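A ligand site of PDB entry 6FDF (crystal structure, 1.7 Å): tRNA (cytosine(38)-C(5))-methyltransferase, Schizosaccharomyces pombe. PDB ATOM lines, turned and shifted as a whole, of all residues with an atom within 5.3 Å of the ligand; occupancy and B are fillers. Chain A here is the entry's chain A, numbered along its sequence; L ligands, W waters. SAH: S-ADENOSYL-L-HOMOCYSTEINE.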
ATOM      1  N   TYR A  17       6.656  23.782 -14.587  1.00  0.00           N
ATOM      2  CA  TYR A  17       6.292  25.164 -14.236  1.00  0.00           C
ATOM      3  C   TYR A  17       5.159  25.157 -13.204  1.00  0.00           C
ATOM      4  O   TYR A  17       4.098  25.747 -13.406  1.00  0.00           O
ATOM      5  CB  TYR A  17       5.882  25.984 -15.473  1.00  0.00           C
ATOM      6  CG  TYR A  17       6.768  25.926 -16.714  1.00  0.00           C
ATOM      7  CD1 TYR A  17       6.587  24.952 -17.686  1.00  0.00           C
ATOM      8  CD2 TYR A  17       7.761  26.889 -16.922  1.00  0.00           C
ATOM      9  CE1 TYR A  17       7.373  24.920 -18.828  1.00  0.00           C
ATOM     10  CE2 TYR A  17       8.561  26.854 -18.062  1.00  0.00           C
ATOM     11  CZ  TYR A  17       8.353  25.872 -19.018  1.00  0.00           C
ATOM     12  OH  TYR A  17       9.111  25.851 -20.158  1.00  0.00           O
ATOM     13  N   SER A  18       5.417  24.449 -12.097  1.00  0.00           N
ATOM     14  CA  SER A  18       4.331  24.040 -11.204  1.00  0.00           C
ATOM     15  C   SER A  18       3.760  25.189 -10.372  1.00  0.00           C
ATOM     16  O   SER A  18       2.590  25.127  -9.966  1.00  0.00           O
ATOM     17  CB  SER A  18       4.820  22.938 -10.269  1.00  0.00           C
ATOM     18  OG  SER A  18       6.138  23.198  -9.814  1.00  0.00           O
ATOM     19  N   GLY A  19       4.550  26.230 -10.101  1.00  0.00           N
ATOM     20  CA  GLY A  19       4.022  27.338  -9.312  1.00  0.00           C
ATOM     21  C   GLY A  19       3.534  26.855  -7.957  1.00  0.00           C
ATOM     22  O   GLY A  19       4.197  26.063  -7.279  1.00  0.00           O
ATOM     23  N   ILE A  20       2.336  27.299  -7.564  1.00  0.00           N
ATOM     24  CA  ILE A  20       1.787  26.849  -6.282  1.00  0.00           C
ATOM     25  C   ILE A  20       0.884  25.638  -6.481  1.00  0.00           C
ATOM     26  O   ILE A  20       0.161  25.228  -5.570  1.00  0.00           O
ATOM     27  CB  ILE A  20       1.034  27.974  -5.563  1.00  0.00           C
ATOM     28  CG1 ILE A  20      -0.154  28.457  -6.396  1.00  0.00           C
ATOM     29  CG2 ILE A  20       1.982  29.129  -5.228  1.00  0.00           C
ATOM     30  CD1 ILE A  20      -1.002  29.520  -5.712  1.00  0.00           C
ATOM     31  N   GLY A  21       0.955  25.008  -7.657  1.00  0.00           N
ATOM     32  CA  GLY A  21       0.275  23.748  -7.849  1.00  0.00           C
ATOM     33  C   GLY A  21      -1.149  23.834  -8.347  1.00  0.00           C
ATOM     34  O   GLY A  21      -1.949  22.936  -8.040  1.00  0.00           O
ATOM     35  N   GLY A  22      -1.498  24.877  -9.103  1.00  0.00           N
ATOM     36  CA  GLY A  22      -2.830  24.928  -9.705  1.00  0.00           C
ATOM     37  C   GLY A  22      -3.192  23.664 -10.444  1.00  0.00           C
ATOM     38  O   GLY A  22      -4.322  23.174 -10.329  1.00  0.00           O
ATOM     39  N   MET A  23      -2.242  23.104 -11.217  1.00  0.00           N
ATOM     40  CA  MET A  23      -2.531  21.887 -11.984  1.00  0.00           C
ATOM     41  C   MET A  23      -2.853  20.717 -11.054  1.00  0.00           C
ATOM     42  O   MET A  23      -3.751  19.922 -11.349  1.00  0.00           O
ATOM     43  CB  MET A  23      -1.352  21.514 -12.882  1.00  0.00           C
ATOM     44  CG  MET A  23      -1.034  22.489 -14.007  1.00  0.00           C
ATOM     45  SD  MET A  23      -2.321  22.478 -15.286  1.00  0.00           S
ATOM     46  CE  MET A  23      -1.590  23.578 -16.486  1.00  0.00           C
ATOM     47  N   ILE A  40       8.105  20.782 -11.025  1.00  0.00           N
ATOM     48  CA  ILE A  40       9.363  21.491 -11.279  1.00  0.00           C
ATOM     49  C   ILE A  40       9.089  22.974 -11.400  1.00  0.00           C
ATOM     50  O   ILE A  40       8.277  23.402 -12.227  1.00  0.00           O
ATOM     51  CB  ILE A  40      10.055  20.959 -12.539  1.00  0.00           C
ATOM     52  CG1 ILE A  40      10.378  19.470 -12.376  1.00  0.00           C
ATOM     53  CG2 ILE A  40      11.330  21.741 -12.806  1.00  0.00           C
ATOM     54  CD1 ILE A  40      11.159  18.891 -13.529  1.00  0.00           C
ATOM     55  N   ASP A  41       9.790  23.768 -10.585  1.00  0.00           N
ATOM     56  CA  ASP A  41       9.730  25.214 -10.672  1.00  0.00           C
ATOM     57  C   ASP A  41      11.045  25.771 -10.150  1.00  0.00           C
ATOM     58  O   ASP A  41      11.640  25.232  -9.224  1.00  0.00           O
ATOM     59  CB  ASP A  41       8.529  25.775  -9.887  1.00  0.00           C
ATOM     60  CG  ASP A  41       8.131  27.175 -10.343  1.00  0.00           C
ATOM     61  OD1 ASP A  41       8.948  28.102 -10.223  1.00  0.00           O
ATOM     62  OD2 ASP A  41       6.990  27.331 -10.825  1.00  0.00           O
ATOM     63  N   ILE A  42      11.480  26.879 -10.757  1.00  0.00           N
ATOM     64  CA  ILE A  42      12.733  27.525 -10.370  1.00  0.00           C
ATOM     65  C   ILE A  42      12.539  28.485  -9.203  1.00  0.00           C
ATOM     66  O   ILE A  42      13.542  28.890  -8.584  1.00  0.00           O
ATOM     67  CB  ILE A  42      13.313  28.244 -11.601  1.00  0.00           C
ATOM     68  CG1 ILE A  42      14.808  28.524 -11.417  1.00  0.00           C
ATOM     69  CG2 ILE A  42      12.534  29.521 -11.910  1.00  0.00           C
ATOM     70  CD1 ILE A  42      15.453  29.136 -12.645  1.00  0.00           C
ATOM     71  N   ASN A  43      11.304  28.833  -8.868  1.00  0.00           N
ATOM     72  CA  ASN A  43      11.017  29.829  -7.837  1.00  0.00           C
ATOM     73  C   ASN A  43      10.904  29.122  -6.496  1.00  0.00           C
ATOM     74  O   ASN A  43       9.926  28.391  -6.273  1.00  0.00           O
ATOM     75  CB  ASN A  43       9.726  30.571  -8.174  1.00  0.00           C
ATOM     76  CG  ASN A  43       9.370  31.665  -7.175  1.00  0.00           C
ATOM     77  OD1 ASN A  43       9.716  31.602  -6.000  1.00  0.00           O
ATOM     78  ND2 ASN A  43       8.672  32.688  -7.648  1.00  0.00           N
ATOM     79  N   ALA A  46       7.516  29.611  -4.674  1.00  0.00           N
ATOM     80  CA  ALA A  46       6.443  28.761  -5.193  1.00  0.00           C
ATOM     81  C   ALA A  46       6.581  27.352  -4.647  1.00  0.00           C
ATOM     82  O   ALA A  46       5.595  26.730  -4.221  1.00  0.00           O
ATOM     83  CB  ALA A  46       6.474  28.746  -6.720  1.00  0.00           C
ATOM     84  N   MET A  61      14.582  23.291 -10.234  1.00  0.00           N
ATOM     85  CA  MET A  61      15.329  22.880 -11.416  1.00  0.00           C
ATOM     86  C   MET A  61      14.975  23.791 -12.578  1.00  0.00           C
ATOM     87  O   MET A  61      13.810  24.147 -12.749  1.00  0.00           O
ATOM     88  CB  MET A  61      15.044  21.421 -11.746  1.00  0.00           C
ATOM     89  CG  MET A  61      15.576  20.935 -13.080  1.00  0.00           C
ATOM     90  SD  MET A  61      15.647  19.142 -13.159  1.00  0.00           S
ATOM     91  CE  MET A  61      14.598  18.659 -11.783  1.00  0.00           C
ATOM     92  N   ASP A  62      15.988  24.156 -13.361  1.00  0.00           N
ATOM     93  CA  ASP A  62      15.795  24.945 -14.579  1.00  0.00           C
ATOM     94  C   ASP A  62      15.324  24.010 -15.686  1.00  0.00           C
ATOM     95  O   ASP A  62      16.086  23.139 -16.129  1.00  0.00           O
ATOM     96  CB  ASP A  62      17.103  25.649 -14.949  1.00  0.00           C
ATOM     97  CG  ASP A  62      16.987  26.485 -16.218  1.00  0.00           C
ATOM     98  OD1 ASP A  62      15.896  26.566 -16.817  1.00  0.00           O
ATOM     99  OD2 ASP A  62      18.017  27.056 -16.621  1.00  0.00           O
ATOM    100  N   ILE A  63      14.082  24.195 -16.144  1.00  0.00           N
ATOM    101  CA  ILE A  63      13.508  23.315 -17.149  1.00  0.00           C
ATOM    102  C   ILE A  63      14.313  23.322 -18.437  1.00  0.00           C
ATOM    103  O   ILE A  63      14.298  22.346 -19.195  1.00  0.00           O
ATOM    104  CB  ILE A  63      12.026  23.710 -17.349  1.00  0.00           C
ATOM    105  CG1 ILE A  63      11.206  23.222 -16.150  1.00  0.00           C
ATOM    106  CG2 ILE A  63      11.445  23.171 -18.664  1.00  0.00           C
ATOM    107  CD1 ILE A  63       9.816  23.789 -16.052  1.00  0.00           C
ATOM    108  N   SER A  64      15.065  24.387 -18.700  1.00  0.00           N
ATOM    109  CA  SER A  64      15.914  24.415 -19.880  1.00  0.00           C
ATOM    110  C   SER A  64      17.083  23.446 -19.806  1.00  0.00           C
ATOM    111  O   SER A  64      17.732  23.198 -20.836  1.00  0.00           O
ATOM    112  CB  SER A  64      16.445  25.821 -20.116  1.00  0.00           C
ATOM    113  OG  SER A  64      17.492  26.102 -19.196  1.00  0.00           O
ATOM    114  N   SER A  82       2.753  25.199 -17.922  1.00  0.00           N
ATOM    115  CA  SER A  82       2.326  26.580 -18.115  1.00  0.00           C
ATOM    116  C   SER A  82       3.605  27.368 -18.397  1.00  0.00           C
ATOM    117  O   SER A  82       4.143  28.061 -17.523  1.00  0.00           O
ATOM    118  CB  SER A  82       1.556  27.123 -16.902  1.00  0.00           C
ATOM    119  OG  SER A  82       0.959  28.371 -17.194  1.00  0.00           O
ATOM    120  N   SER A  84       6.765  29.780 -19.826  1.00  0.00           N
ATOM    121  CA  SER A  84       7.056  31.205 -19.894  1.00  0.00           C
ATOM    122  C   SER A  84       7.543  31.468 -21.319  1.00  0.00           C
ATOM    123  O   SER A  84       8.674  31.134 -21.669  1.00  0.00           O
ATOM    124  CB  SER A  84       8.099  31.610 -18.852  1.00  0.00           C
ATOM    125  OG  SER A  84       8.536  32.944 -19.056  1.00  0.00           O
ATOM    126  N   PRO A 100      18.473  31.129 -20.085  1.00  0.00           N
ATOM    127  CA  PRO A 100      17.396  30.330 -20.687  1.00  0.00           C
ATOM    128  C   PRO A 100      16.059  30.714 -20.080  1.00  0.00           C
ATOM    129  O   PRO A 100      15.734  30.329 -18.950  1.00  0.00           O
ATOM    130  CB  PRO A 100      17.800  28.893 -20.350  1.00  0.00           C
ATOM    131  CG  PRO A 100      19.269  28.925 -20.254  1.00  0.00           C
ATOM    132  CD  PRO A 100      19.624  30.287 -19.688  1.00  0.00           C
ATOM    133  N   ARG A 101      15.256  31.455 -20.850  1.00  0.00           N
ATOM    134  CA  ARG A 101      13.952  31.948 -20.422  1.00  0.00           C
ATOM    135  C   ARG A 101      12.846  31.108 -21.034  1.00  0.00           C
ATOM    136  O   ARG A 101      12.299  30.186 -20.411  1.00  0.00           O
ATOM    137  CB  ARG A 101      13.753  33.393 -20.874  1.00  0.00           C
ATOM    138  CG  ARG A 101      14.930  34.037 -21.643  1.00  0.00           C
ATOM    139  CD  ARG A 101      15.251  33.304 -22.979  1.00  0.00           C
ATOM    140  NE  ARG A 101      15.965  34.074 -24.009  1.00  0.00           N
ATOM    141  CZ  ARG A 101      16.913  34.989 -23.815  1.00  0.00           C
ATOM    142  NH1 ARG A 101      17.376  35.284 -22.608  1.00  0.00           N
ATOM    143  NH2 ARG A 101      17.451  35.588 -24.873  1.00  0.00           N
ATOM    144  N   ALA A 104      13.583  27.354 -22.194  1.00  0.00           N
ATOM    145  CA  ALA A 104      13.067  26.192 -21.483  1.00  0.00           C
ATOM    146  C   ALA A 104      11.926  25.539 -22.256  1.00  0.00           C
ATOM    147  O   ALA A 104      11.885  24.303 -22.351  1.00  0.00           O
ATOM    148  CB  ALA A 104      12.591  26.599 -20.094  1.00  0.00           C
ATOM    149  N   PHE A 292      -9.042  28.153  -6.397  1.00  0.00           N
ATOM    150  CA  PHE A 292      -8.265  27.400  -5.416  1.00  0.00           C
ATOM    151  C   PHE A 292      -9.144  27.053  -4.218  1.00  0.00           C
ATOM    152  O   PHE A 292      -9.987  27.858  -3.807  1.00  0.00           O
ATOM    153  CB  PHE A 292      -7.049  28.203  -4.967  1.00  0.00           C
ATOM    154  CG  PHE A 292      -5.944  28.232  -5.979  1.00  0.00           C
ATOM    155  CD1 PHE A 292      -5.941  29.162  -6.993  1.00  0.00           C
ATOM    156  CD2 PHE A 292      -4.913  27.307  -5.905  1.00  0.00           C
ATOM    157  CE1 PHE A 292      -4.925  29.181  -7.931  1.00  0.00           C
ATOM    158  CE2 PHE A 292      -3.901  27.315  -6.835  1.00  0.00           C
ATOM    159  CZ  PHE A 292      -3.903  28.251  -7.853  1.00  0.00           C
ATOM    160  N   LEU A 311       2.308  35.317  -6.799  1.00  0.00           N
ATOM    161  CA  LEU A 311       2.198  33.924  -7.212  1.00  0.00           C
ATOM    162  C   LEU A 311       0.827  33.659  -7.822  1.00  0.00           C
ATOM    163  O   LEU A 311       0.717  32.938  -8.826  1.00  0.00           O
ATOM    164  CB  LEU A 311       2.450  33.001  -6.023  1.00  0.00           C
ATOM    165  CG  LEU A 311       3.859  33.053  -5.414  1.00  0.00           C
ATOM    166  CD1 LEU A 311       3.963  32.179  -4.168  1.00  0.00           C
ATOM    167  CD2 LEU A 311       4.879  32.629  -6.466  1.00  0.00           C
ATOM    168  N   ASN A 314       0.179  34.822 -11.496  1.00  0.00           N
ATOM    169  CA  ASN A 314       0.716  33.962 -12.545  1.00  0.00           C
ATOM    170  C   ASN A 314       0.108  32.571 -12.552  1.00  0.00           C
ATOM    171  O   ASN A 314       0.629  31.683 -13.222  1.00  0.00           O
ATOM    172  CB  ASN A 314       2.231  33.840 -12.393  1.00  0.00           C
ATOM    173  CG  ASN A 314       2.956  35.098 -12.774  1.00  0.00           C
ATOM    174  OD1 ASN A 314       2.516  35.829 -13.664  1.00  0.00           O
ATOM    175  ND2 ASN A 314       4.067  35.362 -12.104  1.00  0.00           N
ATOM    176  N   SER A 315      -0.979  32.352 -11.809  1.00  0.00           N
ATOM    177  CA  SER A 315      -1.560  31.025 -11.652  1.00  0.00           C
ATOM    178  C   SER A 315      -2.706  30.808 -12.643  1.00  0.00           C
ATOM    179  O   SER A 315      -3.264  31.751 -13.211  1.00  0.00           O
ATOM    180  CB  SER A 315      -2.078  30.826 -10.223  1.00  0.00           C
ATOM    181  OG  SER A 315      -1.014  30.880  -9.283  1.00  0.00           O
ATOM    182  N   ILE A 316      -3.053  29.531 -12.832  1.00  0.00           N
ATOM    183  CA  ILE A 316      -4.171  29.166 -13.700  1.00  0.00           C
ATOM    184  C   ILE A 316      -5.477  29.383 -12.957  1.00  0.00           C
ATOM    185  O   ILE A 316      -5.497  29.607 -11.749  1.00  0.00           O
ATOM    186  CB  ILE A 316      -4.056  27.696 -14.148  1.00  0.00           C
ATOM    187  CG1 ILE A 316      -4.133  26.787 -12.911  1.00  0.00           C
ATOM    188  CG2 ILE A 316      -2.782  27.493 -14.938  1.00  0.00           C
ATOM    189  CD1 ILE A 316      -4.414  25.343 -13.203  1.00  0.00           C
HETATM  190  N   SAH L   1       0.969  27.100 -13.394  1.00  0.00           N
HETATM  191  CA  SAH L   1       1.513  27.464 -12.109  1.00  0.00           C
HETATM  192  CB  SAH L   1       2.363  28.736 -12.193  1.00  0.00           C
HETATM  193  CG  SAH L   1       2.953  28.925 -13.588  1.00  0.00           C
HETATM  194  SD  SAH L   1       3.635  30.537 -13.822  1.00  0.00           S
HETATM  195  C   SAH L   1       0.405  27.619 -11.111  1.00  0.00           C
HETATM  196  O   SAH L   1      -0.755  27.348 -11.478  1.00  0.00           O
HETATM  197  OXT SAH L   1       0.714  28.000  -9.968  1.00  0.00           O
HETATM  198  C5' SAH L   1       5.131  29.984 -14.572  1.00  0.00           C
HETATM  199  C4' SAH L   1       6.018  29.335 -13.511  1.00  0.00           C
HETATM  200  O4' SAH L   1       7.121  28.758 -14.181  1.00  0.00           O
HETATM  201  C3' SAH L   1       6.566  30.324 -12.484  1.00  0.00           C
HETATM  202  O3' SAH L   1       6.310  29.839 -11.165  1.00  0.00           O
HETATM  203  C2' SAH L   1       8.072  30.324 -12.713  1.00  0.00           C
HETATM  204  O2' SAH L   1       8.810  30.360 -11.489  1.00  0.00           O
HETATM  205  C1' SAH L   1       8.302  28.999 -13.432  1.00  0.00           C
HETATM  206  N9  SAH L   1       9.412  29.014 -14.411  1.00  0.00           N
HETATM  207  C8  SAH L   1       9.667  29.944 -15.353  1.00  0.00           C
HETATM  208  N7  SAH L   1      10.775  29.610 -16.064  1.00  0.00           N
HETATM  209  C5  SAH L   1      11.246  28.447 -15.582  1.00  0.00           C
HETATM  210  C6  SAH L   1      12.369  27.540 -15.876  1.00  0.00           C
HETATM  211  N6  SAH L   1      13.249  27.824 -16.863  1.00  0.00           N
HETATM  212  N1  SAH L   1      12.491  26.424 -15.117  1.00  0.00           N
HETATM  213  C2  SAH L   1      11.617  26.123 -14.141  1.00  0.00           C
HETATM  214  N3  SAH L   1      10.570  26.900 -13.806  1.00  0.00           N
HETATM  215  C4  SAH L   1      10.346  28.061 -14.479  1.00  0.00           C
HETATM  216  O   HOH W   1       4.500  31.083  -9.734  1.00  0.00           O
HETATM  217  O   HOH W   2       1.435  24.679 -13.843  1.00  0.00           O
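The side-chain carboxylate of Asp 41 is in hydrogen-bond range of an oxygen (O2') of the ligand (2.6 Å). The backbone NH (N) of Ile 63 sits at hydrogen-bond distance from a nitrogen (N1) of the ligand. A nitrogen (N6) of the ligand is in hydrogen-bond range of the side-chain carboxylate (OD1) of Asp 62, at 2.9 Å. N of Ile 20 lies within hydrogen-bond range of OXT of the ligand. N of Ile 42 lies within hydrogen-bond range of N3 of the ligand (3.2 Å). O of Tyr 17 sits close to N of the ligand (3.4 Å). The side-chain hydroxyl (OG) of Ser 315 lies within hydrogen-bond range of an oxygen (OXT) of the ligand (3.4 Å). The backbone NH (N) of Ile 316 sits at hydrogen-bond distance from an oxygen (O) of the ligand, 3.4 Å away.
N of Gly 19 sits at hydrogen-bond distance from OD2 of Asp 41, at 2.8 Å. The side-chain carboxylate (OD1) of Asp 41 is in hydrogen-bond range of the backbone NH (N) of Asn 43 (2.8 Å). The side-chain hydroxyl (OG) of Ser 64 is in hydrogen-bond range of the side-chain carboxylate (OD2) of Asp 62, at 2.8 Å. O of Ile 40 lies within hydrogen-bond range of N of Tyr 17 (2.9 Å). The backbone carbonyl oxygen (O) of Ile 40 sits at hydrogen-bond distance from the backbone NH (N) of Ser 18 (3.0 Å). The side-chain hydroxyl (OG) of Ser 315 is in hydrogen-bond range of the backbone carbonyl oxygen (O) of Leu 311 (2.7 Å). The side-chain amide oxygen of Asn 43 sits at hydrogen-bond distance from the backbone NH of Ala 46 (3.2 Å).
An oxygen (OXT) of the ligand sits close to the backbone carbonyl oxygen of Ser 18 (3.4 Å). The backbone carbonyl oxygen (O) of Asn 314 lies close to a sulfur (SD) of the ligand. Merely in contact with the ligand: Gly 19, Gly 21, Gly 22, Asn 43, Met 61, Ser 82 and Ala 104. Within 4 Å of the ligand: Tyr 17, Ser 18, Gly 19, Ile 20, Gly 21, Gly 22, Asp 41, Ile 42, Asn 43, Met 61, Asp 62, Ile 63, Ser 82, Ala 104, Asn 314, Ser 315 and Ile 316. Along chain A the residues within 4 Å of the ligand span positions 17 to 316. The nearest printed residue that does not touch the ligand is Pro 100 (4.1 Å).
Water W2 bridges a nitrogen (N) of the ligand (2.5 Å) and the backbone carbonyl oxygen of Tyr 17 (2.9 Å).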
